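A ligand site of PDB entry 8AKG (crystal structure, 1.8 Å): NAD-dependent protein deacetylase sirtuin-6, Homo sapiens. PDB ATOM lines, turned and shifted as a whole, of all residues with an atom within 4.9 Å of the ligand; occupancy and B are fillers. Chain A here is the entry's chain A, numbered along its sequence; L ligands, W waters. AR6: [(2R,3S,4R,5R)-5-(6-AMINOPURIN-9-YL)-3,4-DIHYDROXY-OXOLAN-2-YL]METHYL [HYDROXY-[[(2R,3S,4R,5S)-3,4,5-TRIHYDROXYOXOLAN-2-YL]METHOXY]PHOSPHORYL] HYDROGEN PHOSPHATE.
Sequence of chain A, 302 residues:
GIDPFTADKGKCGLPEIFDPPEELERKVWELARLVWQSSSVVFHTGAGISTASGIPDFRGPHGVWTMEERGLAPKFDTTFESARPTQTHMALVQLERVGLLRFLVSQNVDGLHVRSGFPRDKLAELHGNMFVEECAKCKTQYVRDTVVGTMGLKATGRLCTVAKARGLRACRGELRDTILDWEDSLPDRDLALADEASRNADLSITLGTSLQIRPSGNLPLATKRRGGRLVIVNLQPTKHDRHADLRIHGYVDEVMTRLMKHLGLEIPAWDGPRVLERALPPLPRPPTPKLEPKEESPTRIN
Water W1 lies within hydrogen-bond range of O3D of the ligand (2.6 Å), OD1 of Asn 108 (2.9 Å) and O of Gln 107 (3.2 Å). Water W4 bridges N7 of the ligand and OG1 of Thr 51. Water W2 lies within hydrogen-bond range of the backbone carbonyl oxygen (O) of Gln 107 (2.9 Å) and an oxygen (O3D) of the ligand (3.2 Å). Water W3 lies within hydrogen-bond range of O of Gly 48 (2.9 Å), OG1 of Thr 51 (3.2 Å) and N6 of the ligand (3.4 Å).
The backbone carbonyl oxygen of Gly 48 sits close to a nitrogen (N7) of the ligand (3.3 Å). The backbone carbonyl oxygen (O) of Gly 208 lies close to an oxygen (O4') of the ligand (3.4 Å). Merely in contact with the ligand: Gly 46, Asp 57, Ile 213, Gly 250 and Tyr 251. 20 residues have an atom within 4 Å of the ligand: Gly 46, Ala 47, Gly 48, Thr 51, Asp 57, Phe 58, Arg 59, Trp 65, Gln 107, His 127, Gly 208, Thr 209, Ser 210, Ile 213, Asn 234, Leu 235, Gln 236, Gly 250, Tyr 251 and Val 252. The nearest printed residue that does not touch the ligand is Leu 211 (4.05 Å).
N of Ala 47 sits at hydrogen-bond distance from O1B of the ligand, at 2.9 Å. N of Gln 236 lies close to O2' of the ligand. An oxygen (O1A) of the ligand is in salt-bridge range of the guanidinium group (NH1) of Arg 59 (2.7 Å). An oxygen (O3') of the ligand is in hydrogen-bond range of the side-chain amide nitrogen (ND2) of Asn 234 (2.7 Å). N of Leu 235 is in hydrogen-bond range of N3 of the ligand (3.3 Å). An oxygen (O1A) of the ligand sits at hydrogen-bond distance from the side-chain hydroxyl of Ser 210. A ring nitrogen (ND1) of His 127 sits at hydrogen-bond distance from an oxygen (O3D) of the ligand (2.8 Å). An oxygen (O2A) of the ligand sits at hydrogen-bond distance from the backbone NH (N) of Phe 58 (2.9 Å). N of Arg 59 is in hydrogen-bond range of O2A of the ligand (2.8 Å). The side-chain amide oxygen (OE1) of Gln 236 sits at hydrogen-bond distance from an oxygen (O3') of the ligand (2.7 Å). O3D of the ligand sits at hydrogen-bond distance from O of Gln 107, at 2.8 Å. N1 of the ligand sits at hydrogen-bond distance from N of Val 252, at 2.9 Å. The backbone NH (N) of Ser 210 is in hydrogen-bond range of an oxygen (O2B) of the ligand (3.2 Å). N7 of the ligand is in hydrogen-bond range of OG1 of Thr 51, 2.8 Å away. NE1 of Trp 65 lies within hydrogen-bond range of O1D of the ligand (3.3 Å). The side-chain hydroxyl of Thr 209 sits at hydrogen-bond distance from an oxygen (O2B) of the ligand (2.8 Å).
The backbone carbonyl oxygen (O) of Arg 59 sits at hydrogen-bond distance from the side-chain amide nitrogen (NE2) of Gln 236 (2.9 Å). The side-chain amide nitrogen (NE2) of Gln 212 is in hydrogen-bond range of the side-chain hydroxyl (OG) of Ser 210, 3.2 Å away. O of Phe 58 sits at hydrogen-bond distance from N of Trp 65, 2.9 Å away. The side-chain amide oxygen (OD1) of Asn 108 sits at hydrogen-bond distance from the backbone NH (N) of Ala 47, 3.0 Å away. The side-chain hydroxyl (OG1) of Thr 209 sits at hydrogen-bond distance from the backbone NH (N) of Leu 211 (3.1 Å). O of Gly 208 lies within hydrogen-bond range of N of Gly 48 (2.9 Å). The side-chain amide oxygen (OD1) of Asn 234 is in hydrogen-bond range of the backbone NH (N) of Thr 209 (3.1 Å). The side-chain amide nitrogen of Asn 234 is in hydrogen-bond range of the backbone carbonyl oxygen of Gln 236, at 3.0 Å.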
ATOM      1  N   GLU A  16      26.219  -4.555  19.700  1.00  0.00           N
ATOM      2  CA  GLU A  16      26.260  -3.849  21.010  1.00  0.00           C
ATOM      3  C   GLU A  16      26.857  -2.459  20.798  1.00  0.00           C
ATOM      4  O   GLU A  16      27.744  -2.285  19.917  1.00  0.00           O
ATOM      5  CB  GLU A  16      27.047  -4.689  22.002  1.00  0.00           C
ATOM      6  CG  GLU A  16      26.370  -6.001  22.306  1.00  0.00           C
ATOM      7  CD  GLU A  16      26.955  -6.738  23.474  1.00  0.00           C
ATOM      8  OE1 GLU A  16      28.197  -6.749  23.579  1.00  0.00           O
ATOM      9  OE2 GLU A  16      26.166  -7.289  24.271  1.00  0.00           O
ATOM     10  N   GLY A  46      14.113  -6.779  31.685  1.00  0.00           N
ATOM     11  CA  GLY A  46      14.114  -7.931  30.783  1.00  0.00           C
ATOM     12  C   GLY A  46      15.359  -8.740  31.002  1.00  0.00           C
ATOM     13  O   GLY A  46      16.038  -8.501  32.050  1.00  0.00           O
ATOM     14  N   ALA A  47      15.656  -9.645  30.067  1.00  0.00           N
ATOM     15  CA  ALA A  47      16.655 -10.725  30.238  1.00  0.00           C
ATOM     16  C   ALA A  47      18.047 -10.151  30.499  1.00  0.00           C
ATOM     17  O   ALA A  47      18.869 -10.864  31.152  1.00  0.00           O
ATOM     18  CB  ALA A  47      16.678 -11.624  29.012  1.00  0.00           C
ATOM     19  N   GLY A  48      18.301  -8.934  30.020  1.00  0.00           N
ATOM     20  CA  GLY A  48      19.605  -8.261  30.141  1.00  0.00           C
ATOM     21  C   GLY A  48      20.012  -8.093  31.585  1.00  0.00           C
ATOM     22  O   GLY A  48      21.224  -8.051  31.829  1.00  0.00           O
ATOM     23  N   THR A  51      21.862 -11.593  32.845  1.00  0.00           N
ATOM     24  CA  THR A  51      22.997 -12.161  32.069  1.00  0.00           C
ATOM     25  C   THR A  51      24.247 -12.258  32.946  1.00  0.00           C
ATOM     26  O   THR A  51      25.007 -13.238  32.756  1.00  0.00           O
ATOM     27  CB  THR A  51      23.296 -11.401  30.767  1.00  0.00           C
ATOM     28  OG1 THR A  51      23.542 -10.018  31.027  1.00  0.00           O
ATOM     29  CG2 THR A  51      22.212 -11.552  29.713  1.00  0.00           C
ATOM     30  N   ASP A  57      20.544 -14.049  27.689  1.00  0.00           N
ATOM     31  CA  ASP A  57      19.308 -13.361  27.229  1.00  0.00           C
ATOM     32  C   ASP A  57      18.745 -14.033  25.975  1.00  0.00           C
ATOM     33  O   ASP A  57      19.162 -15.131  25.601  1.00  0.00           O
ATOM     34  CB  ASP A  57      19.576 -11.874  27.011  1.00  0.00           C
ATOM     35  CG  ASP A  57      20.611 -11.519  25.943  1.00  0.00           C
ATOM     36  OD1 ASP A  57      20.868 -12.324  25.019  1.00  0.00           O
ATOM     37  OD2 ASP A  57      21.180 -10.440  26.067  1.00  0.00           O
ATOM     38  N   PHE A  58      17.731 -13.424  25.383  1.00  0.00           N
ATOM     39  CA  PHE A  58      17.049 -13.952  24.178  1.00  0.00           C
ATOM     40  C   PHE A  58      17.733 -13.425  22.907  1.00  0.00           C
ATOM     41  O   PHE A  58      17.992 -14.264  22.048  1.00  0.00           O
ATOM     42  CB  PHE A  58      15.551 -13.662  24.271  1.00  0.00           C
ATOM     43  CG  PHE A  58      14.883 -14.452  25.367  1.00  0.00           C
ATOM     44  CD1 PHE A  58      14.444 -15.746  25.141  1.00  0.00           C
ATOM     45  CD2 PHE A  58      14.703 -13.906  26.637  1.00  0.00           C
ATOM     46  CE1 PHE A  58      13.846 -16.491  26.138  1.00  0.00           C
ATOM     47  CE2 PHE A  58      14.076 -14.644  27.629  1.00  0.00           C
ATOM     48  CZ  PHE A  58      13.632 -15.930  27.383  1.00  0.00           C
ATOM     49  N   ARG A  59      18.021 -12.128  22.784  1.00  0.00           N
ATOM     50  CA  ARG A  59      18.312 -11.499  21.460  1.00  0.00           C
ATOM     51  C   ARG A  59      19.670 -10.770  21.461  1.00  0.00           C
ATOM     52  O   ARG A  59      20.046 -10.217  20.392  1.00  0.00           O
ATOM     53  CB  ARG A  59      17.187 -10.552  21.034  1.00  0.00           C
ATOM     54  CG  ARG A  59      15.836 -11.234  20.931  1.00  0.00           C
ATOM     55  CD  ARG A  59      14.695 -10.313  20.557  1.00  0.00           C
ATOM     56  NE  ARG A  59      13.470 -11.056  20.616  1.00  0.00           N
ATOM     57  CZ  ARG A  59      12.741 -11.342  21.694  1.00  0.00           C
ATOM     58  NH1 ARG A  59      13.046 -10.899  22.910  1.00  0.00           N
ATOM     59  NH2 ARG A  59      11.657 -12.084  21.530  1.00  0.00           N
ATOM     60  N   GLY A  60      20.450 -10.898  22.547  1.00  0.00           N
ATOM     61  CA  GLY A  60      21.857 -10.459  22.576  1.00  0.00           C
ATOM     62  C   GLY A  60      22.746 -11.283  21.649  1.00  0.00           C
ATOM     63  O   GLY A  60      22.335 -12.303  21.097  1.00  0.00           O
ATOM     64  N   TRP A  65      17.447 -17.056  21.302  1.00  0.00           N
ATOM     65  CA  TRP A  65      16.933 -16.901  19.913  1.00  0.00           C
ATOM     66  C   TRP A  65      18.075 -16.622  18.911  1.00  0.00           C
ATOM     67  O   TRP A  65      18.120 -17.281  17.842  1.00  0.00           O
ATOM     68  CB  TRP A  65      15.852 -15.803  19.824  1.00  0.00           C
ATOM     69  CG  TRP A  65      14.648 -15.949  20.702  1.00  0.00           C
ATOM     70  CD1 TRP A  65      13.839 -14.919  21.078  1.00  0.00           C
ATOM     71  CD2 TRP A  65      14.065 -17.134  21.262  1.00  0.00           C
ATOM     72  NE1 TRP A  65      12.805 -15.375  21.856  1.00  0.00           N
ATOM     73  CE2 TRP A  65      12.929 -16.723  21.998  1.00  0.00           C
ATOM     74  CE3 TRP A  65      14.397 -18.500  21.256  1.00  0.00           C
ATOM     75  CZ2 TRP A  65      12.123 -17.622  22.692  1.00  0.00           C
ATOM     76  CZ3 TRP A  65      13.596 -19.386  21.943  1.00  0.00           C
ATOM     77  CH2 TRP A  65      12.479 -18.951  22.660  1.00  0.00           C
ATOM     78  N   GLN A 107       9.565  -8.762  32.385  1.00  0.00           N
ATOM     79  CA  GLN A 107       9.335  -9.794  31.357  1.00  0.00           C
ATOM     80  C   GLN A 107      10.085 -11.072  31.727  1.00  0.00           C
ATOM     81  O   GLN A 107       9.878 -12.073  31.048  1.00  0.00           O
ATOM     82  CB  GLN A 107       9.794  -9.205  30.029  1.00  0.00           C
ATOM     83  CG  GLN A 107       8.988  -8.009  29.554  1.00  0.00           C
ATOM     84  CD  GLN A 107       9.606  -7.444  28.300  1.00  0.00           C
ATOM     85  OE1 GLN A 107       9.532  -8.044  27.221  1.00  0.00           O
ATOM     86  NE2 GLN A 107      10.285  -6.321  28.455  1.00  0.00           N
ATOM     87  N   ASN A 108      10.881 -11.051  32.811  1.00  0.00           N
ATOM     88  CA  ASN A 108      11.720 -12.199  33.222  1.00  0.00           C
ATOM     89  C   ASN A 108      10.864 -13.246  33.932  1.00  0.00           C
ATOM     90  O   ASN A 108      10.056 -12.864  34.847  1.00  0.00           O
ATOM     91  CB  ASN A 108      12.908 -11.750  34.084  1.00  0.00           C
ATOM     92  CG  ASN A 108      13.860 -10.868  33.302  1.00  0.00           C
ATOM     93  OD1 ASN A 108      13.678 -10.664  32.117  1.00  0.00           O
ATOM     94  ND2 ASN A 108      14.870 -10.339  33.974  1.00  0.00           N
ATOM     95  N   HIS A 127       5.321 -12.247  31.974  1.00  0.00           N
ATOM     96  CA  HIS A 127       5.473 -13.528  31.229  1.00  0.00           C
ATOM     97  C   HIS A 127       5.477 -14.722  32.198  1.00  0.00           C
ATOM     98  O   HIS A 127       5.705 -15.876  31.749  1.00  0.00           O
ATOM     99  CB  HIS A 127       6.702 -13.436  30.308  1.00  0.00           C
ATOM    100  CG  HIS A 127       6.666 -12.240  29.407  1.00  0.00           C
ATOM    101  ND1 HIS A 127       7.784 -11.758  28.722  1.00  0.00           N
ATOM    102  CD2 HIS A 127       5.637 -11.416  29.094  1.00  0.00           C
ATOM    103  CE1 HIS A 127       7.437 -10.710  28.032  1.00  0.00           C
ATOM    104  NE2 HIS A 127       6.126 -10.482  28.227  1.00  0.00           N
ATOM    105  N   TRP A 182       3.455 -18.912  23.481  1.00  0.00           N
ATOM    106  CA  TRP A 182       3.401 -17.822  22.466  1.00  0.00           C
ATOM    107  C   TRP A 182       1.967 -17.286  22.351  1.00  0.00           C
ATOM    108  O   TRP A 182       1.817 -16.064  22.303  1.00  0.00           O
ATOM    109  CB  TRP A 182       3.957 -18.328  21.128  1.00  0.00           C
ATOM    110  CG  TRP A 182       5.444 -18.497  21.156  1.00  0.00           C
ATOM    111  CD1 TRP A 182       6.139 -19.648  21.414  1.00  0.00           C
ATOM    112  CD2 TRP A 182       6.425 -17.471  20.977  1.00  0.00           C
ATOM    113  NE1 TRP A 182       7.489 -19.402  21.379  1.00  0.00           N
ATOM    114  CE2 TRP A 182       7.694 -18.078  21.104  1.00  0.00           C
ATOM    115  CE3 TRP A 182       6.353 -16.092  20.695  1.00  0.00           C
ATOM    116  CZ2 TRP A 182       8.874 -17.355  20.974  1.00  0.00           C
ATOM    117  CZ3 TRP A 182       7.532 -15.385  20.549  1.00  0.00           C
ATOM    118  CH2 TRP A 182       8.773 -16.005  20.697  1.00  0.00           C
ATOM    119  N   GLY A 208      17.960  -3.725  30.389  1.00  0.00           N
ATOM    120  CA  GLY A 208      18.165  -5.018  29.739  1.00  0.00           C
ATOM    121  C   GLY A 208      16.938  -5.553  29.046  1.00  0.00           C
ATOM    122  O   GLY A 208      16.702  -6.735  29.153  1.00  0.00           O
ATOM    123  N   THR A 209      16.199  -4.693  28.362  1.00  0.00           N
ATOM    124  CA  THR A 209      15.116  -5.166  27.454  1.00  0.00           C
ATOM    125  C   THR A 209      15.244  -4.461  26.093  1.00  0.00           C
ATOM    126  O   THR A 209      15.510  -3.278  26.058  1.00  0.00           O
ATOM    127  CB  THR A 209      13.724  -5.095  28.096  1.00  0.00           C
ATOM    128  OG1 THR A 209      12.751  -5.394  27.097  1.00  0.00           O
ATOM    129  CG2 THR A 209      13.438  -3.759  28.729  1.00  0.00           C
ATOM    130  N   SER A 210      15.068  -5.224  25.012  1.00  0.00           N
ATOM    131  CA  SER A 210      15.077  -4.724  23.623  1.00  0.00           C
ATOM    132  C   SER A 210      13.688  -4.199  23.278  1.00  0.00           C
ATOM    133  O   SER A 210      13.576  -3.567  22.245  1.00  0.00           O
ATOM    134  CB  SER A 210      15.593  -5.775  22.651  1.00  0.00           C
ATOM    135  OG  SER A 210      14.757  -6.895  22.568  1.00  0.00           O
ATOM    136  N   LEU A 211      12.669  -4.465  24.120  1.00  0.00           N
ATOM    137  CA  LEU A 211      11.325  -3.795  24.037  1.00  0.00           C
ATOM    138  C   LEU A 211      10.572  -4.232  22.768  1.00  0.00           C
ATOM    139  O   LEU A 211       9.776  -3.423  22.227  1.00  0.00           O
ATOM    140  CB  LEU A 211      11.505  -2.271  24.089  1.00  0.00           C
ATOM    141  CG  LEU A 211      12.187  -1.715  25.335  1.00  0.00           C
ATOM    142  CD1 LEU A 211      12.508  -0.233  25.160  1.00  0.00           C
ATOM    143  CD2 LEU A 211      11.332  -1.939  26.574  1.00  0.00           C
ATOM    144  N   GLN A 212      10.781  -5.460  22.323  1.00  0.00           N
ATOM    145  CA  GLN A 212      10.272  -5.978  21.034  1.00  0.00           C
ATOM    146  C   GLN A 212       8.928  -6.676  21.241  1.00  0.00           C
ATOM    147  O   GLN A 212       8.262  -6.887  20.226  1.00  0.00           O
ATOM    148  CB  GLN A 212      11.288  -6.925  20.412  1.00  0.00           C
ATOM    149  CG  GLN A 212      12.622  -6.252  20.099  1.00  0.00           C
ATOM    150  CD  GLN A 212      13.413  -7.047  19.114  1.00  0.00           C
ATOM    151  OE1 GLN A 212      12.915  -7.405  18.061  1.00  0.00           O
ATOM    152  NE2 GLN A 212      14.706  -7.241  19.399  1.00  0.00           N
ATOM    153  N   ILE A 213       8.568  -7.055  22.476  1.00  0.00           N
ATOM    154  CA  ILE A 213       7.318  -7.824  22.768  1.00  0.00           C
ATOM    155  C   ILE A 213       6.186  -6.838  23.074  1.00  0.00           C
ATOM    156  O   ILE A 213       6.346  -6.015  24.030  1.00  0.00           O
ATOM    157  CB  ILE A 213       7.549  -8.823  23.919  1.00  0.00           C
ATOM    158  CG1 ILE A 213       8.552  -9.919  23.537  1.00  0.00           C
ATOM    159  CG2 ILE A 213       6.232  -9.407  24.394  1.00  0.00           C
ATOM    160  CD1 ILE A 213       8.052 -10.902  22.512  1.00  0.00           C
ATOM    161  N   ASN A 234      20.476  -0.277  27.945  1.00  0.00           N
ATOM    162  CA  ASN A 234      20.599  -1.464  27.073  1.00  0.00           C
ATOM    163  C   ASN A 234      21.885  -1.401  26.264  1.00  0.00           C
ATOM    164  O   ASN A 234      22.242  -0.313  25.726  1.00  0.00           O
ATOM    165  CB  ASN A 234      19.401  -1.622  26.129  1.00  0.00           C
ATOM    166  CG  ASN A 234      19.077  -3.075  25.924  1.00  0.00           C
ATOM    167  OD1 ASN A 234      18.754  -3.798  26.866  1.00  0.00           O
ATOM    168  ND2 ASN A 234      19.130  -3.523  24.687  1.00  0.00           N
ATOM    169  N   LEU A 235      22.542  -2.553  26.125  1.00  0.00           N
ATOM    170  CA  LEU A 235      23.774  -2.642  25.287  1.00  0.00           C
ATOM    171  C   LEU A 235      23.448  -2.559  23.792  1.00  0.00           C
ATOM    172  O   LEU A 235      24.270  -1.946  23.076  1.00  0.00           O
ATOM    173  CB  LEU A 235      24.527  -3.918  25.649  1.00  0.00           C
ATOM    174  CG  LEU A 235      25.287  -3.845  26.965  1.00  0.00           C
ATOM    175  CD1 LEU A 235      25.795  -5.211  27.346  1.00  0.00           C
ATOM    176  CD2 LEU A 235      26.439  -2.836  26.865  1.00  0.00           C
ATOM    177  N   GLN A 236      22.320  -3.144  23.365  1.00  0.00           N
ATOM    178  CA  GLN A 236      21.841  -3.201  21.949  1.00  0.00           C
ATOM    179  C   GLN A 236      20.846  -2.067  21.775  1.00  0.00           C
ATOM    180  O   GLN A 236      20.327  -1.526  22.756  1.00  0.00           O
ATOM    181  CB  GLN A 236      21.117  -4.514  21.595  1.00  0.00           C
ATOM    182  CG  GLN A 236      22.011  -5.728  21.385  1.00  0.00           C
ATOM    183  CD  GLN A 236      21.260  -7.018  21.161  1.00  0.00           C
ATOM    184  OE1 GLN A 236      20.244  -7.322  21.808  1.00  0.00           O
ATOM    185  NE2 GLN A 236      21.767  -7.854  20.255  1.00  0.00           N
ATOM    186  N   PRO A 237      20.554  -1.679  20.524  1.00  0.00           N
ATOM    187  CA  PRO A 237      19.404  -0.842  20.207  1.00  0.00           C
ATOM    188  C   PRO A 237      18.113  -1.543  20.662  1.00  0.00           C
ATOM    189  O   PRO A 237      18.059  -2.762  20.748  1.00  0.00           O
ATOM    190  CB  PRO A 237      19.453  -0.647  18.687  1.00  0.00           C
ATOM    191  CG  PRO A 237      20.851  -1.087  18.285  1.00  0.00           C
ATOM    192  CD  PRO A 237      21.300  -2.084  19.317  1.00  0.00           C
ATOM    193  N   GLY A 250      25.585   0.593  28.183  1.00  0.00           N
ATOM    194  CA  GLY A 250      26.533   0.075  29.186  1.00  0.00           C
ATOM    195  C   GLY A 250      25.936  -1.094  29.920  1.00  0.00           C
ATOM    196  O   GLY A 250      24.738  -1.354  29.708  1.00  0.00           O
ATOM    197  N   TYR A 251      26.747  -1.836  30.658  1.00  0.00           N
ATOM    198  CA  TYR A 251      26.305  -3.005  31.462  1.00  0.00           C
ATOM    199  C   TYR A 251      25.400  -2.467  32.564  1.00  0.00           C
ATOM    200  O   TYR A 251      25.794  -1.456  33.205  1.00  0.00           O
ATOM    201  CB  TYR A 251      27.506  -3.759  32.032  1.00  0.00           C
ATOM    202  CG  TYR A 251      28.310  -4.429  30.961  1.00  0.00           C
ATOM    203  CD1 TYR A 251      27.935  -5.663  30.448  1.00  0.00           C
ATOM    204  CD2 TYR A 251      29.450  -3.830  30.448  1.00  0.00           C
ATOM    205  CE1 TYR A 251      28.674  -6.287  29.461  1.00  0.00           C
ATOM    206  CE2 TYR A 251      30.187  -4.437  29.445  1.00  0.00           C
ATOM    207  CZ  TYR A 251      29.798  -5.665  28.952  1.00  0.00           C
ATOM    208  OH  TYR A 251      30.520  -6.274  27.966  1.00  0.00           O
ATOM    209  N   VAL A 252      24.190  -3.020  32.687  1.00  0.00           N
ATOM    210  CA  VAL A 252      23.199  -2.495  33.656  1.00  0.00           C
ATOM    211  C   VAL A 252      23.824  -2.534  35.055  1.00  0.00           C
ATOM    212  O   VAL A 252      23.563  -1.604  35.813  1.00  0.00           O
ATOM    213  CB  VAL A 252      21.811  -3.116  33.553  1.00  0.00           C
ATOM    214  CG1 VAL A 252      21.804  -4.637  33.792  1.00  0.00           C
ATOM    215  CG2 VAL A 252      20.863  -2.395  34.498  1.00  0.00           C
HETATM  216  N1  AR6 L   1      23.688  -4.883  30.544  1.00  0.00           N
HETATM  217  C2  AR6 L   1      22.912  -4.218  29.672  1.00  0.00           C
HETATM  218  N3  AR6 L   1      22.191  -4.688  28.659  1.00  0.00           N
HETATM  219  C4  AR6 L   1      22.288  -6.032  28.591  1.00  0.00           C
HETATM  220  C5  AR6 L   1      23.051  -6.842  29.393  1.00  0.00           C
HETATM  221  C6  AR6 L   1      23.807  -6.227  30.407  1.00  0.00           C
HETATM  222  N6  AR6 L   1      24.563  -6.897  31.272  1.00  0.00           N
HETATM  223  N7  AR6 L   1      22.896  -8.152  29.006  1.00  0.00           N
HETATM  224  C8  AR6 L   1      22.047  -8.126  28.000  1.00  0.00           C
HETATM  225  N9  AR6 L   1      21.680  -6.864  27.685  1.00  0.00           N
HETATM  226  PA  AR6 L   1      16.065  -9.555  24.887  1.00  0.00           P
HETATM  227  PB  AR6 L   1      13.758  -9.237  26.634  1.00  0.00           P
HETATM  228  C1' AR6 L   1      20.714  -6.434  26.725  1.00  0.00           C
HETATM  229  O1A AR6 L   1      15.144  -9.358  23.746  1.00  0.00           O
HETATM  230  O1B AR6 L   1      13.519  -9.303  28.105  1.00  0.00           O
HETATM  231  C1D AR6 L   1      11.272 -13.521  24.868  1.00  0.00           C
HETATM  232  O1D AR6 L   1      10.511 -14.288  23.978  1.00  0.00           O
HETATM  233  C2' AR6 L   1      20.814  -6.977  25.307  1.00  0.00           C
HETATM  234  O2' AR6 L   1      21.620  -6.106  24.573  1.00  0.00           O
HETATM  235  O2A AR6 L   1      17.147 -10.579  24.891  1.00  0.00           O
HETATM  236  O2B AR6 L   1      13.601  -7.889  26.063  1.00  0.00           O
HETATM  237  C2D AR6 L   1      10.703 -13.792  26.270  1.00  0.00           C
HETATM  238  O2D AR6 L   1       9.307 -14.080  26.205  1.00  0.00           O
HETATM  239  C3' AR6 L   1      19.358  -7.028  24.829  1.00  0.00           C
HETATM  240  O3' AR6 L   1      18.959  -6.062  23.885  1.00  0.00           O
HETATM  241  O3A AR6 L   1      15.183  -9.871  26.220  1.00  0.00           O
HETATM  242  C3D AR6 L   1      11.087 -12.507  26.996  1.00  0.00           C
HETATM  243  O3D AR6 L   1      10.453 -12.277  28.271  1.00  0.00           O
HETATM  244  C4' AR6 L   1      18.545  -6.958  26.129  1.00  0.00           C
HETATM  245  O4' AR6 L   1      19.477  -6.882  27.230  1.00  0.00           O
HETATM  246  C4D AR6 L   1      10.715 -11.485  25.915  1.00  0.00           C
HETATM  247  O4D AR6 L   1      11.098 -12.120  24.666  1.00  0.00           O
HETATM  248  C5' AR6 L   1      17.683  -8.157  26.337  1.00  0.00           C
HETATM  249  O5' AR6 L   1      16.707  -8.174  25.275  1.00  0.00           O
HETATM  250  C5D AR6 L   1      11.380 -10.128  25.999  1.00  0.00           C
HETATM  251  O5D AR6 L   1      12.822 -10.294  25.921  1.00  0.00           O
HETATM  252  O   HOH W   1      12.611 -11.498  29.569  1.00  0.00           O
HETATM  253  O   HOH W   2      11.732 -14.286  30.477  1.00  0.00           O
HETATM  254  O   HOH W   3      23.227  -8.532  33.886  1.00  0.00           O
HETATM  255  O   HOH W   4      25.204  -9.481  28.146  1.00  0.00           O
HETATM  256  O   HOH W   5       7.915 -14.181  23.499  1.00  0.00           O
HETATM  257  O   HOH W   6      25.213  -6.158  34.119  1.00  0.00           O
HETATM  258  O   HOH W   7      23.614  -9.916  25.630  1.00  0.00           O
HETATM  259  O   HOH W   8      12.410  -7.612  23.643  1.00  0.00           O
